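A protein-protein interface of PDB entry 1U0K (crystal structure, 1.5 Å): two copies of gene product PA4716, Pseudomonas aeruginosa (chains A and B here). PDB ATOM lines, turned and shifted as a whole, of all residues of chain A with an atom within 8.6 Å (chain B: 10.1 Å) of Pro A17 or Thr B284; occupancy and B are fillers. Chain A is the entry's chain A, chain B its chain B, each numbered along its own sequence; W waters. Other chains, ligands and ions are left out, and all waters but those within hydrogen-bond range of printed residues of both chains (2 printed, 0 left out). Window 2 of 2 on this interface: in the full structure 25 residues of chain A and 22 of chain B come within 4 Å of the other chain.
The side-chain carboxylate (OE2) of Glu B43 sits at hydrogen-bond distance from the side-chain amide nitrogen (NE2) of Gln A9 (2.9 Å). OD1 of Asp A11 sits close to OE2 of Glu B43 (2.5 Å). NH2 of Arg A254 is in salt-bridge range of OE1 of Glu B43 (3.0 Å). The backbone NH of Leu B283 sits at hydrogen-bond distance from the backbone carbonyl oxygen of Leu A277 (2.8 Å). N of Glu B281 lies within hydrogen-bond range of O of Arg A279 (2.8 Å).
The side-chain carboxylate (OD2) of Asp A11 sits at hydrogen-bond distance from the backbone NH (N) of Leu A18 (2.9 Å). The backbone carbonyl oxygen (O) of Thr A19 is in hydrogen-bond range of the guanidinium group (NH2) of Arg A254 (3.1 Å). The guanidinium group (NE) of Arg A254 lies within hydrogen-bond range of the backbone carbonyl oxygen (O) of Gly A20. OG of Ser B4 is in hydrogen-bond range of O of Leu B282 (3.0 Å). O of Thr B284 lies within hydrogen-bond range of N of Ser B4 (3.1 Å). The backbone carbonyl oxygen (O) of Arg B5 lies within hydrogen-bond range of the backbone NH (N) of Leu B282.
No position is printed for both chains. Of the 16 pairs that touch across the chains among the printed residues, none has its exchanged pair printed and touching as well.
Among the printed residues, merely in contact across the chains: Pro A17 with Thr B284 (3.4 Å), Leu A18 with Glu B43 (3.6 Å), Leu A276 with Leu B283 (3.8 Å), Leu A277 with Glu B43 (3.3 Å), Leu A277 with Leu B282 (3.5 Å), Leu A277 with Thr B284 (3.8 Å), Ala A278 with Tyr B7 (3.8 Å), Ala A278 with Glu B281 (3.3 Å), Ala A278 with Leu B283 (3.8 Å), Arg A279 with Ala B280 (3.4 Å) and Arg A279 with Leu B283 (3.7 Å).
Hydrophobic or aromatic side chains of chain B within 4 Å of the printed part of chain A: Tyr B7 and Leu B283. Hydrophobic or aromatic side chains of chain A that line the printed part of chain B: Pro A17, Leu A18, Leu A277 and Ala A278. Among the printed residues, Asp or Glu carboxylates within 4 Å of a Lys or Arg side-chain nitrogen of the other chain: Arg A254 with Glu B43 (3.0 Å).
Of chain B, only Thr B284 (3.4 Å) comes within 4 Å of Pro A17. Of chain A, only Pro A17 (3.4 Å) and Leu A277 (3.8 Å) come within 4 Å of Thr B284. No residue of chain B comes within 4 Å of Thr A19. Leu A277 touches four residues of chain B. Printed residues of chain B within 4 Å of Asp A11: Glu B43. Of the printed residues of chain A, Leu B282 touches Leu A277 (3.5 Å). The nearest residue of chain B that does not touch Pro A17 is Ser B285 (4.9 Å). The nearest residue of chain A that does not touch Thr B284 is Leu A276 (4.5 Å).
Water W1 lies within hydrogen-bond range of O of Leu B283 (2.7 Å) and O of Leu A276 (2.7 Å). Water W2 bridges the backbone carbonyl oxygen of Ala B39 (2.7 Å) and the guanidinium group of Arg A254 (3.3 Å).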
ATOM      1  N   GLN A   9     -10.066 -23.382  20.828  1.00  0.00           N
ATOM      2  CA  GLN A   9     -10.883 -24.570  20.665  1.00  0.00           C
ATOM      3  C   GLN A   9     -11.243 -24.702  19.197  1.00  0.00           C
ATOM      4  O   GLN A   9     -11.787 -23.788  18.608  1.00  0.00           O
ATOM      5  CB  GLN A   9     -12.157 -24.467  21.528  1.00  0.00           C
ATOM      6  CG  GLN A   9     -13.121 -25.626  21.381  1.00  0.00           C
ATOM      7  CD  GLN A   9     -12.563 -26.951  21.860  1.00  0.00           C
ATOM      8  OE1 GLN A   9     -11.629 -26.988  22.668  1.00  0.00           O
ATOM      9  NE2 GLN A   9     -13.125 -28.041  21.356  1.00  0.00           N
ATOM     10  N   LEU A  10     -10.870 -25.828  18.602  1.00  0.00           N
ATOM     11  CA  LEU A  10     -11.101 -26.119  17.191  1.00  0.00           C
ATOM     12  C   LEU A  10     -11.810 -27.453  17.054  1.00  0.00           C
ATOM     13  O   LEU A  10     -11.730 -28.292  17.939  1.00  0.00           O
ATOM     14  CB  LEU A  10      -9.761 -26.231  16.444  1.00  0.00           C
ATOM     15  CG  LEU A  10      -9.047 -24.950  16.028  1.00  0.00           C
ATOM     16  CD1 LEU A  10      -8.596 -24.131  17.192  1.00  0.00           C
ATOM     17  CD2 LEU A  10      -7.855 -25.302  15.154  1.00  0.00           C
ATOM     18  N   ASP A  11     -12.464 -27.658  15.920  1.00  0.00           N
ATOM     19  CA  ASP A  11     -12.914 -28.986  15.522  1.00  0.00           C
ATOM     20  C   ASP A  11     -12.198 -29.418  14.261  1.00  0.00           C
ATOM     21  O   ASP A  11     -12.128 -28.662  13.298  1.00  0.00           O
ATOM     22  CB  ASP A  11     -14.406 -28.980  15.250  1.00  0.00           C
ATOM     23  CG  ASP A  11     -15.213 -28.860  16.497  1.00  0.00           C
ATOM     24  OD1 ASP A  11     -14.779 -29.376  17.557  1.00  0.00           O
ATOM     25  OD2 ASP A  11     -16.296 -28.256  16.512  1.00  0.00           O
ATOM     26  N   VAL A  12     -11.690 -30.646  14.272  1.00  0.00           N
ATOM     27  CA  VAL A  12     -10.962 -31.206  13.136  1.00  0.00           C
ATOM     28  C   VAL A  12     -11.787 -32.343  12.520  1.00  0.00           C
ATOM     29  O   VAL A  12     -12.462 -33.098  13.237  1.00  0.00           O
ATOM     30  CB  VAL A  12      -9.582 -31.727  13.576  1.00  0.00           C
ATOM     31  CG1 VAL A  12      -8.778 -32.237  12.366  1.00  0.00           C
ATOM     32  CG2 VAL A  12      -8.798 -30.639  14.323  1.00  0.00           C
ATOM     33  N   ALA A  14     -14.249 -31.569  10.375  1.00  0.00           N
ATOM     34  CA  ALA A  14     -15.495 -30.879  10.686  1.00  0.00           C
ATOM     35  C   ALA A  14     -15.775 -29.826   9.623  1.00  0.00           C
ATOM     36  O   ALA A  14     -15.013 -28.873   9.459  1.00  0.00           O
ATOM     37  CB  ALA A  14     -15.396 -30.224  12.080  1.00  0.00           C
ATOM     38  N   GLU A  15     -16.869 -29.996   8.884  1.00  0.00           N
ATOM     39  CA  GLU A  15     -17.274 -29.002   7.903  1.00  0.00           C
ATOM     40  C   GLU A  15     -18.170 -27.929   8.515  1.00  0.00           C
ATOM     41  O   GLU A  15     -18.362 -26.880   7.909  1.00  0.00           O
ATOM     42  CB  GLU A  15     -17.945 -29.669   6.700  1.00  0.00           C
ATOM     43  CG  GLU A  15     -17.017 -30.672   6.032  1.00  0.00           C
ATOM     44  CD  GLU A  15     -17.447 -31.129   4.654  1.00  0.00           C
ATOM     45  OE1 GLU A  15     -17.244 -32.332   4.352  1.00  0.00           O
ATOM     46  OE2 GLU A  15     -17.950 -30.303   3.861  1.00  0.00           O
ATOM     47  N   ARG A  16     -18.706 -28.199   9.706  1.00  0.00           N
ATOM     48  CA  ARG A  16     -19.434 -27.206  10.497  1.00  0.00           C
ATOM     49  C   ARG A  16     -18.956 -27.235  11.950  1.00  0.00           C
ATOM     50  O   ARG A  16     -18.462 -28.250  12.416  1.00  0.00           O
ATOM     51  CB  ARG A  16     -20.929 -27.512  10.486  1.00  0.00           C
ATOM     52  CG  ARG A  16     -21.604 -27.317   9.151  1.00  0.00           C
ATOM     53  CD  ARG A  16     -23.108 -27.494   9.223  1.00  0.00           C
ATOM     54  NE  ARG A  16     -23.465 -28.742   9.890  1.00  0.00           N
ATOM     55  CZ  ARG A  16     -23.530 -29.930   9.295  1.00  0.00           C
ATOM     56  NH1 ARG A  16     -23.276 -30.064   7.999  1.00  0.00           N
ATOM     57  NH2 ARG A  16     -23.861 -30.998  10.006  1.00  0.00           N
ATOM     58  N   PRO A  17     -19.118 -26.137  12.679  1.00  0.00           N
ATOM     59  CA  PRO A  17     -18.759 -26.132  14.101  1.00  0.00           C
ATOM     60  C   PRO A  17     -19.583 -27.120  14.920  1.00  0.00           C
ATOM     61  O   PRO A  17     -20.712 -27.453  14.544  1.00  0.00           O
ATOM     62  CB  PRO A  17     -19.053 -24.698  14.547  1.00  0.00           C
ATOM     63  CG  PRO A  17     -19.889 -24.100  13.483  1.00  0.00           C
ATOM     64  CD  PRO A  17     -19.621 -24.828  12.228  1.00  0.00           C
ATOM     65  N   LEU A  18     -19.023 -27.555  16.044  1.00  0.00           N
ATOM     66  CA  LEU A  18     -19.666 -28.520  16.944  1.00  0.00           C
ATOM     67  C   LEU A  18     -19.917 -29.879  16.301  1.00  0.00           C
ATOM     68  O   LEU A  18     -20.888 -30.571  16.626  1.00  0.00           O
ATOM     69  CB  LEU A  18     -20.960 -27.940  17.528  1.00  0.00           C
ATOM     70  CG  LEU A  18     -20.806 -26.540  18.131  1.00  0.00           C
ATOM     71  CD1 LEU A  18     -22.160 -25.876  18.325  1.00  0.00           C
ATOM     72  CD2 LEU A  18     -20.070 -26.616  19.446  1.00  0.00           C
ATOM     73  N   THR A  19     -19.028 -30.246  15.375  1.00  0.00           N
ATOM     74  CA  THR A  19     -18.967 -31.592  14.817  1.00  0.00           C
ATOM     75  C   THR A  19     -17.503 -32.033  14.788  1.00  0.00           C
ATOM     76  O   THR A  19     -16.615 -31.262  15.133  1.00  0.00           O
ATOM     77  CB  THR A  19     -19.550 -31.637  13.383  1.00  0.00           C
ATOM     78  OG1 THR A  19     -18.734 -30.870  12.484  1.00  0.00           O
ATOM     79  CG2 THR A  19     -20.914 -30.977  13.306  1.00  0.00           C
ATOM     80  N   GLY A  20     -17.251 -33.263  14.358  1.00  0.00           N
ATOM     81  CA  GLY A  20     -15.888 -33.743  14.244  1.00  0.00           C
ATOM     82  C   GLY A  20     -15.203 -33.866  15.590  1.00  0.00           C
ATOM     83  O   GLY A  20     -15.846 -34.026  16.627  1.00  0.00           O
ATOM     84  N   SER A 116     -16.370 -21.356   6.040  1.00  0.00           N
ATOM     85  CA  SER A 116     -16.257 -20.722   7.356  1.00  0.00           C
ATOM     86  C   SER A 116     -14.924 -21.035   8.060  1.00  0.00           C
ATOM     87  O   SER A 116     -14.560 -20.386   9.062  1.00  0.00           O
ATOM     88  CB  SER A 116     -17.426 -21.155   8.255  1.00  0.00           C
ATOM     89  OG  SER A 116     -17.550 -22.577   8.322  1.00  0.00           O
ATOM     90  N   GLY A 117     -14.197 -22.023   7.547  1.00  0.00           N
ATOM     91  CA  GLY A 117     -12.957 -22.440   8.173  1.00  0.00           C
ATOM     92  C   GLY A 117     -11.838 -22.714   7.194  1.00  0.00           C
ATOM     93  O   GLY A 117     -11.507 -21.869   6.355  1.00  0.00           O
ATOM     94  N   ARG A 254     -21.006 -38.283  16.308  1.00  0.00           N
ATOM     95  CA  ARG A 254     -20.153 -37.293  15.655  1.00  0.00           C
ATOM     96  C   ARG A 254     -19.498 -37.922  14.421  1.00  0.00           C
ATOM     97  O   ARG A 254     -18.270 -38.028  14.340  1.00  0.00           O
ATOM     98  CB  ARG A 254     -19.097 -36.764  16.636  1.00  0.00           C
ATOM     99  CG  ARG A 254     -19.662 -35.716  17.592  1.00  0.00           C
ATOM    100  CD  ARG A 254     -18.728 -35.303  18.709  1.00  0.00           C
ATOM    101  NE  ARG A 254     -17.908 -34.144  18.346  1.00  0.00           N
ATOM    102  CZ  ARG A 254     -18.279 -32.864  18.464  1.00  0.00           C
ATOM    103  NH1 ARG A 254     -19.460 -32.531  18.964  1.00  0.00           N
ATOM    104  NH2 ARG A 254     -17.437 -31.900  18.101  1.00  0.00           N
ATOM    105  N   VAL A 274     -11.383 -28.011   9.030  1.00  0.00           N
ATOM    106  CA  VAL A 274     -11.151 -27.536  10.384  1.00  0.00           C
ATOM    107  C   VAL A 274     -11.946 -26.262  10.624  1.00  0.00           C
ATOM    108  O   VAL A 274     -11.945 -25.364   9.795  1.00  0.00           O
ATOM    109  CB  VAL A 274      -9.653 -27.248  10.628  1.00  0.00           C
ATOM    110  CG1 VAL A 274      -9.433 -26.765  12.058  1.00  0.00           C
ATOM    111  CG2 VAL A 274      -8.804 -28.490  10.323  1.00  0.00           C
ATOM    112  N   GLN A 275     -12.631 -26.205  11.762  1.00  0.00           N
ATOM    113  CA  GLN A 275     -13.353 -25.021  12.191  1.00  0.00           C
ATOM    114  C   GLN A 275     -12.745 -24.470  13.469  1.00  0.00           C
ATOM    115  O   GLN A 275     -12.336 -25.230  14.332  1.00  0.00           O
ATOM    116  CB  GLN A 275     -14.815 -25.370  12.471  1.00  0.00           C
ATOM    117  CG  GLN A 275     -15.511 -26.087  11.334  1.00  0.00           C
ATOM    118  CD  GLN A 275     -15.492 -25.307  10.025  1.00  0.00           C
ATOM    119  OE1 GLN A 275     -15.766 -24.107   9.997  1.00  0.00           O
ATOM    120  NE2 GLN A 275     -15.169 -25.993   8.942  1.00  0.00           N
ATOM    121  N   LEU A 276     -12.732 -23.149  13.597  1.00  0.00           N
ATOM    122  CA  LEU A 276     -12.273 -22.474  14.806  1.00  0.00           C
ATOM    123  C   LEU A 276     -13.499 -22.025  15.608  1.00  0.00           C
ATOM    124  O   LEU A 276     -14.364 -21.327  15.086  1.00  0.00           O
ATOM    125  CB  LEU A 276     -11.400 -21.280  14.447  1.00  0.00           C
ATOM    126  CG  LEU A 276      -9.924 -21.531  14.143  1.00  0.00           C
ATOM    127  CD1 LEU A 276      -9.754 -22.430  12.940  1.00  0.00           C
ATOM    128  CD2 LEU A 276      -9.224 -20.200  13.920  1.00  0.00           C
ATOM    129  N   LEU A 277     -13.579 -22.448  16.860  1.00  0.00           N
ATOM    130  CA  LEU A 277     -14.773 -22.221  17.685  1.00  0.00           C
ATOM    131  C   LEU A 277     -14.638 -21.132  18.743  1.00  0.00           C
ATOM    132  O   LEU A 277     -15.610 -20.420  18.999  1.00  0.00           O
ATOM    133  CB  LEU A 277     -15.181 -23.518  18.380  1.00  0.00           C
ATOM    134  CG  LEU A 277     -16.072 -24.469  17.584  1.00  0.00           C
ATOM    135  CD1 LEU A 277     -15.448 -24.975  16.301  1.00  0.00           C
ATOM    136  CD2 LEU A 277     -16.470 -25.629  18.485  1.00  0.00           C
ATOM    137  N   ALA A 278     -13.482 -21.031  19.391  1.00  0.00           N
ATOM    138  CA  ALA A 278     -13.293 -20.104  20.508  1.00  0.00           C
ATOM    139  C   ALA A 278     -11.836 -19.743  20.690  1.00  0.00           C
ATOM    140  O   ALA A 278     -10.936 -20.550  20.425  1.00  0.00           O
ATOM    141  CB  ALA A 278     -13.823 -20.701  21.801  1.00  0.00           C
ATOM    142  N   ARG A 279     -11.604 -18.517  21.131  1.00  0.00           N
ATOM    143  CA  ARG A 279     -10.299 -18.010  21.503  1.00  0.00           C
ATOM    144  C   ARG A 279     -10.330 -17.680  22.997  1.00  0.00           C
ATOM    145  O   ARG A 279     -11.134 -16.854  23.425  1.00  0.00           O
ATOM    146  CB  ARG A 279      -9.982 -16.729  20.713  1.00  0.00           C
ATOM    147  CG  ARG A 279      -8.632 -16.103  21.015  1.00  0.00           C
ATOM    148  CD  ARG A 279      -8.438 -14.718  20.390  1.00  0.00           C
ATOM    149  NE  ARG A 279      -9.387 -13.760  20.962  1.00  0.00           N
ATOM    150  CZ  ARG A 279     -10.393 -13.184  20.308  1.00  0.00           C
ATOM    151  NH1 ARG A 279     -10.631 -13.451  19.028  1.00  0.00           N
ATOM    152  NH2 ARG A 279     -11.191 -12.339  20.955  1.00  0.00           N
ATOM    153  N   SER B   4     -21.691 -16.123  18.553  1.00  0.00           N
ATOM    154  CA  SER B   4     -20.653 -15.347  19.296  1.00  0.00           C
ATOM    155  C   SER B   4     -21.133 -14.842  20.668  1.00  0.00           C
ATOM    156  O   SER B   4     -22.185 -14.227  20.792  1.00  0.00           O
ATOM    157  CB  SER B   4     -20.132 -14.189  18.446  1.00  0.00           C
ATOM    158  OG  SER B   4     -19.021 -14.602  17.658  1.00  0.00           O
ATOM    159  N   ARG B   5     -20.330 -15.145  21.688  1.00  0.00           N
ATOM    160  CA  ARG B   5     -20.453 -14.621  23.042  1.00  0.00           C
ATOM    161  C   ARG B   5     -19.287 -15.126  23.893  1.00  0.00           C
ATOM    162  O   ARG B   5     -18.166 -15.139  23.416  1.00  0.00           O
ATOM    163  CB  ARG B   5     -21.815 -14.877  23.702  1.00  0.00           C
ATOM    164  CG  ARG B   5     -22.469 -16.245  23.540  1.00  0.00           C
ATOM    165  CD  ARG B   5     -23.991 -16.172  23.603  1.00  0.00           C
ATOM    166  NE  ARG B   5     -24.484 -14.844  23.187  1.00  0.00           N
ATOM    167  CZ  ARG B   5     -24.563 -13.762  23.977  1.00  0.00           C
ATOM    168  NH1 ARG B   5     -24.204 -13.817  25.256  1.00  0.00           N
ATOM    169  NH2 ARG B   5     -24.999 -12.614  23.480  1.00  0.00           N
ATOM    170  N   ARG B   6     -19.534 -15.535  25.133  1.00  0.00           N
ATOM    171  CA  ARG B   6     -18.472 -15.582  26.138  1.00  0.00           C
ATOM    172  C   ARG B   6     -18.683 -16.740  27.100  1.00  0.00           C
ATOM    173  O   ARG B   6     -19.786 -16.968  27.541  1.00  0.00           O
ATOM    174  CB  ARG B   6     -18.489 -14.269  26.936  1.00  0.00           C
ATOM    175  CG  ARG B   6     -17.380 -14.105  27.920  1.00  0.00           C
ATOM    176  CD  ARG B   6     -17.214 -12.689  28.366  1.00  0.00           C
ATOM    177  NE  ARG B   6     -18.268 -12.292  29.288  1.00  0.00           N
ATOM    178  CZ  ARG B   6     -18.327 -11.102  29.868  1.00  0.00           C
ATOM    179  NH1 ARG B   6     -17.416 -10.185  29.578  1.00  0.00           N
ATOM    180  NH2 ARG B   6     -19.289 -10.820  30.730  1.00  0.00           N
ATOM    181  N   TYR B   7     -17.622 -17.468  27.425  1.00  0.00           N
ATOM    182  CA  TYR B   7     -17.660 -18.347  28.583  1.00  0.00           C
ATOM    183  C   TYR B   7     -16.325 -18.272  29.297  1.00  0.00           C
ATOM    184  O   TYR B   7     -15.351 -17.739  28.771  1.00  0.00           O
ATOM    185  CB  TYR B   7     -18.010 -19.795  28.201  1.00  0.00           C
ATOM    186  CG  TYR B   7     -16.932 -20.513  27.417  1.00  0.00           C
ATOM    187  CD1 TYR B   7     -15.914 -21.234  28.048  1.00  0.00           C
ATOM    188  CD2 TYR B   7     -16.926 -20.462  26.037  1.00  0.00           C
ATOM    189  CE1 TYR B   7     -14.940 -21.887  27.307  1.00  0.00           C
ATOM    190  CE2 TYR B   7     -15.966 -21.109  25.294  1.00  0.00           C
ATOM    191  CZ  TYR B   7     -14.973 -21.815  25.924  1.00  0.00           C
ATOM    192  OH  TYR B   7     -14.018 -22.425  25.130  1.00  0.00           O
ATOM    193  N   PHE B  26     -21.074 -19.959  31.274  1.00  0.00           N
ATOM    194  CA  PHE B  26     -21.572 -18.965  30.318  1.00  0.00           C
ATOM    195  C   PHE B  26     -22.331 -17.918  31.132  1.00  0.00           C
ATOM    196  O   PHE B  26     -23.376 -18.229  31.704  1.00  0.00           O
ATOM    197  CB  PHE B  26     -22.474 -19.639  29.291  1.00  0.00           C
ATOM    198  CG  PHE B  26     -21.738 -20.488  28.278  1.00  0.00           C
ATOM    199  CD1 PHE B  26     -21.155 -21.691  28.649  1.00  0.00           C
ATOM    200  CD2 PHE B  26     -21.637 -20.089  26.960  1.00  0.00           C
ATOM    201  CE1 PHE B  26     -20.475 -22.470  27.714  1.00  0.00           C
ATOM    202  CE2 PHE B  26     -20.962 -20.878  26.029  1.00  0.00           C
ATOM    203  CZ  PHE B  26     -20.382 -22.063  26.426  1.00  0.00           C
ATOM    204  N   LEU B  32     -29.324 -18.491  24.188  1.00  0.00           N
ATOM    205  CA  LEU B  32     -28.992 -19.873  23.872  1.00  0.00           C
ATOM    206  C   LEU B  32     -30.174 -20.762  24.165  1.00  0.00           C
ATOM    207  O   LEU B  32     -30.642 -20.803  25.301  1.00  0.00           O
ATOM    208  CB  LEU B  32     -27.804 -20.362  24.706  1.00  0.00           C
ATOM    209  CG  LEU B  32     -26.453 -19.698  24.481  1.00  0.00           C
ATOM    210  CD1 LEU B  32     -25.416 -20.339  25.391  1.00  0.00           C
ATOM    211  CD2 LEU B  32     -26.027 -19.786  23.030  1.00  0.00           C
ATOM    212  N   ALA B  36     -28.563 -25.749  22.260  1.00  0.00           N
ATOM    213  CA  ALA B  36     -27.270 -25.084  22.128  1.00  0.00           C
ATOM    214  C   ALA B  36     -26.492 -25.215  23.424  1.00  0.00           C
ATOM    215  O   ALA B  36     -25.277 -25.424  23.398  1.00  0.00           O
ATOM    216  CB  ALA B  36     -27.428 -23.628  21.763  1.00  0.00           C
ATOM    217  N   ALA B  39     -25.212 -28.708  23.452  1.00  0.00           N
ATOM    218  CA  ALA B  39     -24.175 -28.877  22.425  1.00  0.00           C
ATOM    219  C   ALA B  39     -22.845 -28.280  22.869  1.00  0.00           C
ATOM    220  O   ALA B  39     -21.786 -28.900  22.664  1.00  0.00           O
ATOM    221  CB  ALA B  39     -24.622 -28.295  21.113  1.00  0.00           C
ATOM    222  N   TRP B  40     -22.875 -27.105  23.488  1.00  0.00           N
ATOM    223  CA  TRP B  40     -21.633 -26.486  23.969  1.00  0.00           C
ATOM    224  C   TRP B  40     -21.077 -27.282  25.125  1.00  0.00           C
ATOM    225  O   TRP B  40     -19.870 -27.427  25.252  1.00  0.00           O
ATOM    226  CB  TRP B  40     -21.836 -25.014  24.367  1.00  0.00           C
ATOM    227  CG  TRP B  40     -21.750 -24.124  23.191  1.00  0.00           C
ATOM    228  CD1 TRP B  40     -22.776 -23.475  22.573  1.00  0.00           C
ATOM    229  CD2 TRP B  40     -20.574 -23.797  22.465  1.00  0.00           C
ATOM    230  NE1 TRP B  40     -22.303 -22.759  21.498  1.00  0.00           N
ATOM    231  CE2 TRP B  40     -20.950 -22.952  21.404  1.00  0.00           C
ATOM    232  CE3 TRP B  40     -19.225 -24.149  22.595  1.00  0.00           C
ATOM    233  CZ2 TRP B  40     -20.027 -22.443  20.491  1.00  0.00           C
ATOM    234  CZ3 TRP B  40     -18.315 -23.645  21.689  1.00  0.00           C
ATOM    235  CH2 TRP B  40     -18.720 -22.806  20.648  1.00  0.00           C
ATOM    236  N   GLU B  43     -19.234 -30.082  23.577  1.00  0.00           N
ATOM    237  CA  GLU B  43     -18.034 -29.594  22.905  1.00  0.00           C
ATOM    238  C   GLU B  43     -16.896 -29.391  23.894  1.00  0.00           C
ATOM    239  O   GLU B  43     -15.750 -29.814  23.642  1.00  0.00           O
ATOM    240  CB  GLU B  43     -18.309 -28.280  22.173  1.00  0.00           C
ATOM    241  CG  GLU B  43     -17.123 -27.761  21.371  1.00  0.00           C
ATOM    242  CD  GLU B  43     -16.738 -28.642  20.211  1.00  0.00           C
ATOM    243  OE1 GLU B  43     -17.573 -29.413  19.694  1.00  0.00           O
ATOM    244  OE2 GLU B  43     -15.561 -28.523  19.792  1.00  0.00           O
ATOM    245  N   LEU B  44     -17.194 -28.722  25.004  1.00  0.00           N
ATOM    246  CA  LEU B  44     -16.160 -28.321  25.960  1.00  0.00           C
ATOM    247  C   LEU B  44     -15.700 -29.460  26.859  1.00  0.00           C
ATOM    248  O   LEU B  44     -14.621 -29.396  27.422  1.00  0.00           O
ATOM    249  CB  LEU B  44     -16.638 -27.124  26.792  1.00  0.00           C
ATOM    250  CG  LEU B  44     -16.956 -25.872  25.970  1.00  0.00           C
ATOM    251  CD1 LEU B  44     -17.409 -24.765  26.896  1.00  0.00           C
ATOM    252  CD2 LEU B  44     -15.761 -25.419  25.143  1.00  0.00           C
ATOM    253  N   ALA B 280     -13.009 -16.954  27.478  1.00  0.00           N
ATOM    254  CA  ALA B 280     -13.127 -17.453  26.107  1.00  0.00           C
ATOM    255  C   ALA B 280     -14.185 -16.688  25.325  1.00  0.00           C
ATOM    256  O   ALA B 280     -15.271 -16.414  25.827  1.00  0.00           O
ATOM    257  CB  ALA B 280     -13.453 -18.934  26.108  1.00  0.00           C
ATOM    258  N   GLU B 281     -13.840 -16.291  24.112  1.00  0.00           N
ATOM    259  CA  GLU B 281     -14.768 -15.604  23.227  1.00  0.00           C
ATOM    260  C   GLU B 281     -15.102 -16.538  22.076  1.00  0.00           C
ATOM    261  O   GLU B 281     -14.190 -17.098  21.459  1.00  0.00           O
ATOM    262  CB  GLU B 281     -14.119 -14.320  22.706  1.00  0.00           C
ATOM    263  CG  GLU B 281     -13.650 -13.350  23.792  1.00  0.00           C
ATOM    264  CD  GLU B 281     -14.781 -12.709  24.588  1.00  0.00           C
ATOM    265  OE1 GLU B 281     -15.887 -12.500  24.032  1.00  0.00           O
ATOM    266  OE2 GLU B 281     -14.564 -12.413  25.793  1.00  0.00           O
ATOM    267  N   LEU B 282     -16.386 -16.744  21.804  1.00  0.00           N
ATOM    268  CA  LEU B 282     -16.802 -17.584  20.690  1.00  0.00           C
ATOM    269  C   LEU B 282     -16.499 -16.911  19.357  1.00  0.00           C
ATOM    270  O   LEU B 282     -16.670 -15.701  19.200  1.00  0.00           O
ATOM    271  CB  LEU B 282     -18.292 -17.945  20.764  1.00  0.00           C
ATOM    272  CG  LEU B 282     -18.787 -18.665  22.021  1.00  0.00           C
ATOM    273  CD1 LEU B 282     -20.238 -19.092  21.800  1.00  0.00           C
ATOM    274  CD2 LEU B 282     -17.908 -19.851  22.404  1.00  0.00           C
ATOM    275  N   LEU B 283     -16.055 -17.736  18.409  1.00  0.00           N
ATOM    276  CA  LEU B 283     -15.706 -17.325  17.048  1.00  0.00           C
ATOM    277  C   LEU B 283     -16.719 -17.871  16.032  1.00  0.00           C
ATOM    278  O   LEU B 283     -16.511 -17.759  14.820  1.00  0.00           O
ATOM    279  CB  LEU B 283     -14.309 -17.849  16.703  1.00  0.00           C
ATOM    280  CG  LEU B 283     -13.157 -17.451  17.628  1.00  0.00           C
ATOM    281  CD1 LEU B 283     -11.877 -18.190  17.222  1.00  0.00           C
ATOM    282  CD2 LEU B 283     -12.941 -15.970  17.595  1.00  0.00           C
ATOM    283  N   THR B 284     -17.796 -18.478  16.522  1.00  0.00           N
ATOM    284  CA  THR B 284     -18.889 -18.955  15.673  1.00  0.00           C
ATOM    285  C   THR B 284     -20.235 -18.749  16.356  1.00  0.00           C
ATOM    286  O   THR B 284     -20.331 -18.781  17.579  1.00  0.00           O
ATOM    287  CB  THR B 284     -18.734 -20.451  15.339  1.00  0.00           C
ATOM    288  OG1 THR B 284     -19.892 -20.906  14.623  1.00  0.00           O
ATOM    289  CG2 THR B 284     -18.729 -21.310  16.604  1.00  0.00           C
ATOM    290  N   SER B 285     -21.273 -18.576  15.541  1.00  0.00           N
ATOM    291  CA  SER B 285     -22.645 -18.433  16.017  1.00  0.00           C
ATOM    292  C   SER B 285     -23.455 -19.682  15.668  1.00  0.00           C
ATOM    293  O   SER B 285     -22.910 -20.720  15.258  1.00  0.00           O
ATOM    294  CB  SER B 285     -23.281 -17.185  15.399  1.00  0.00           C
ATOM    295  OG  SER B 285     -22.925 -17.057  14.031  1.00  0.00           O
HETATM  296  O   HOH W   1     -14.825 -19.253  13.361  1.00  0.00           O
HETATM  297  O   HOH W   2     -21.665 -30.668  20.590  1.00  0.00           O
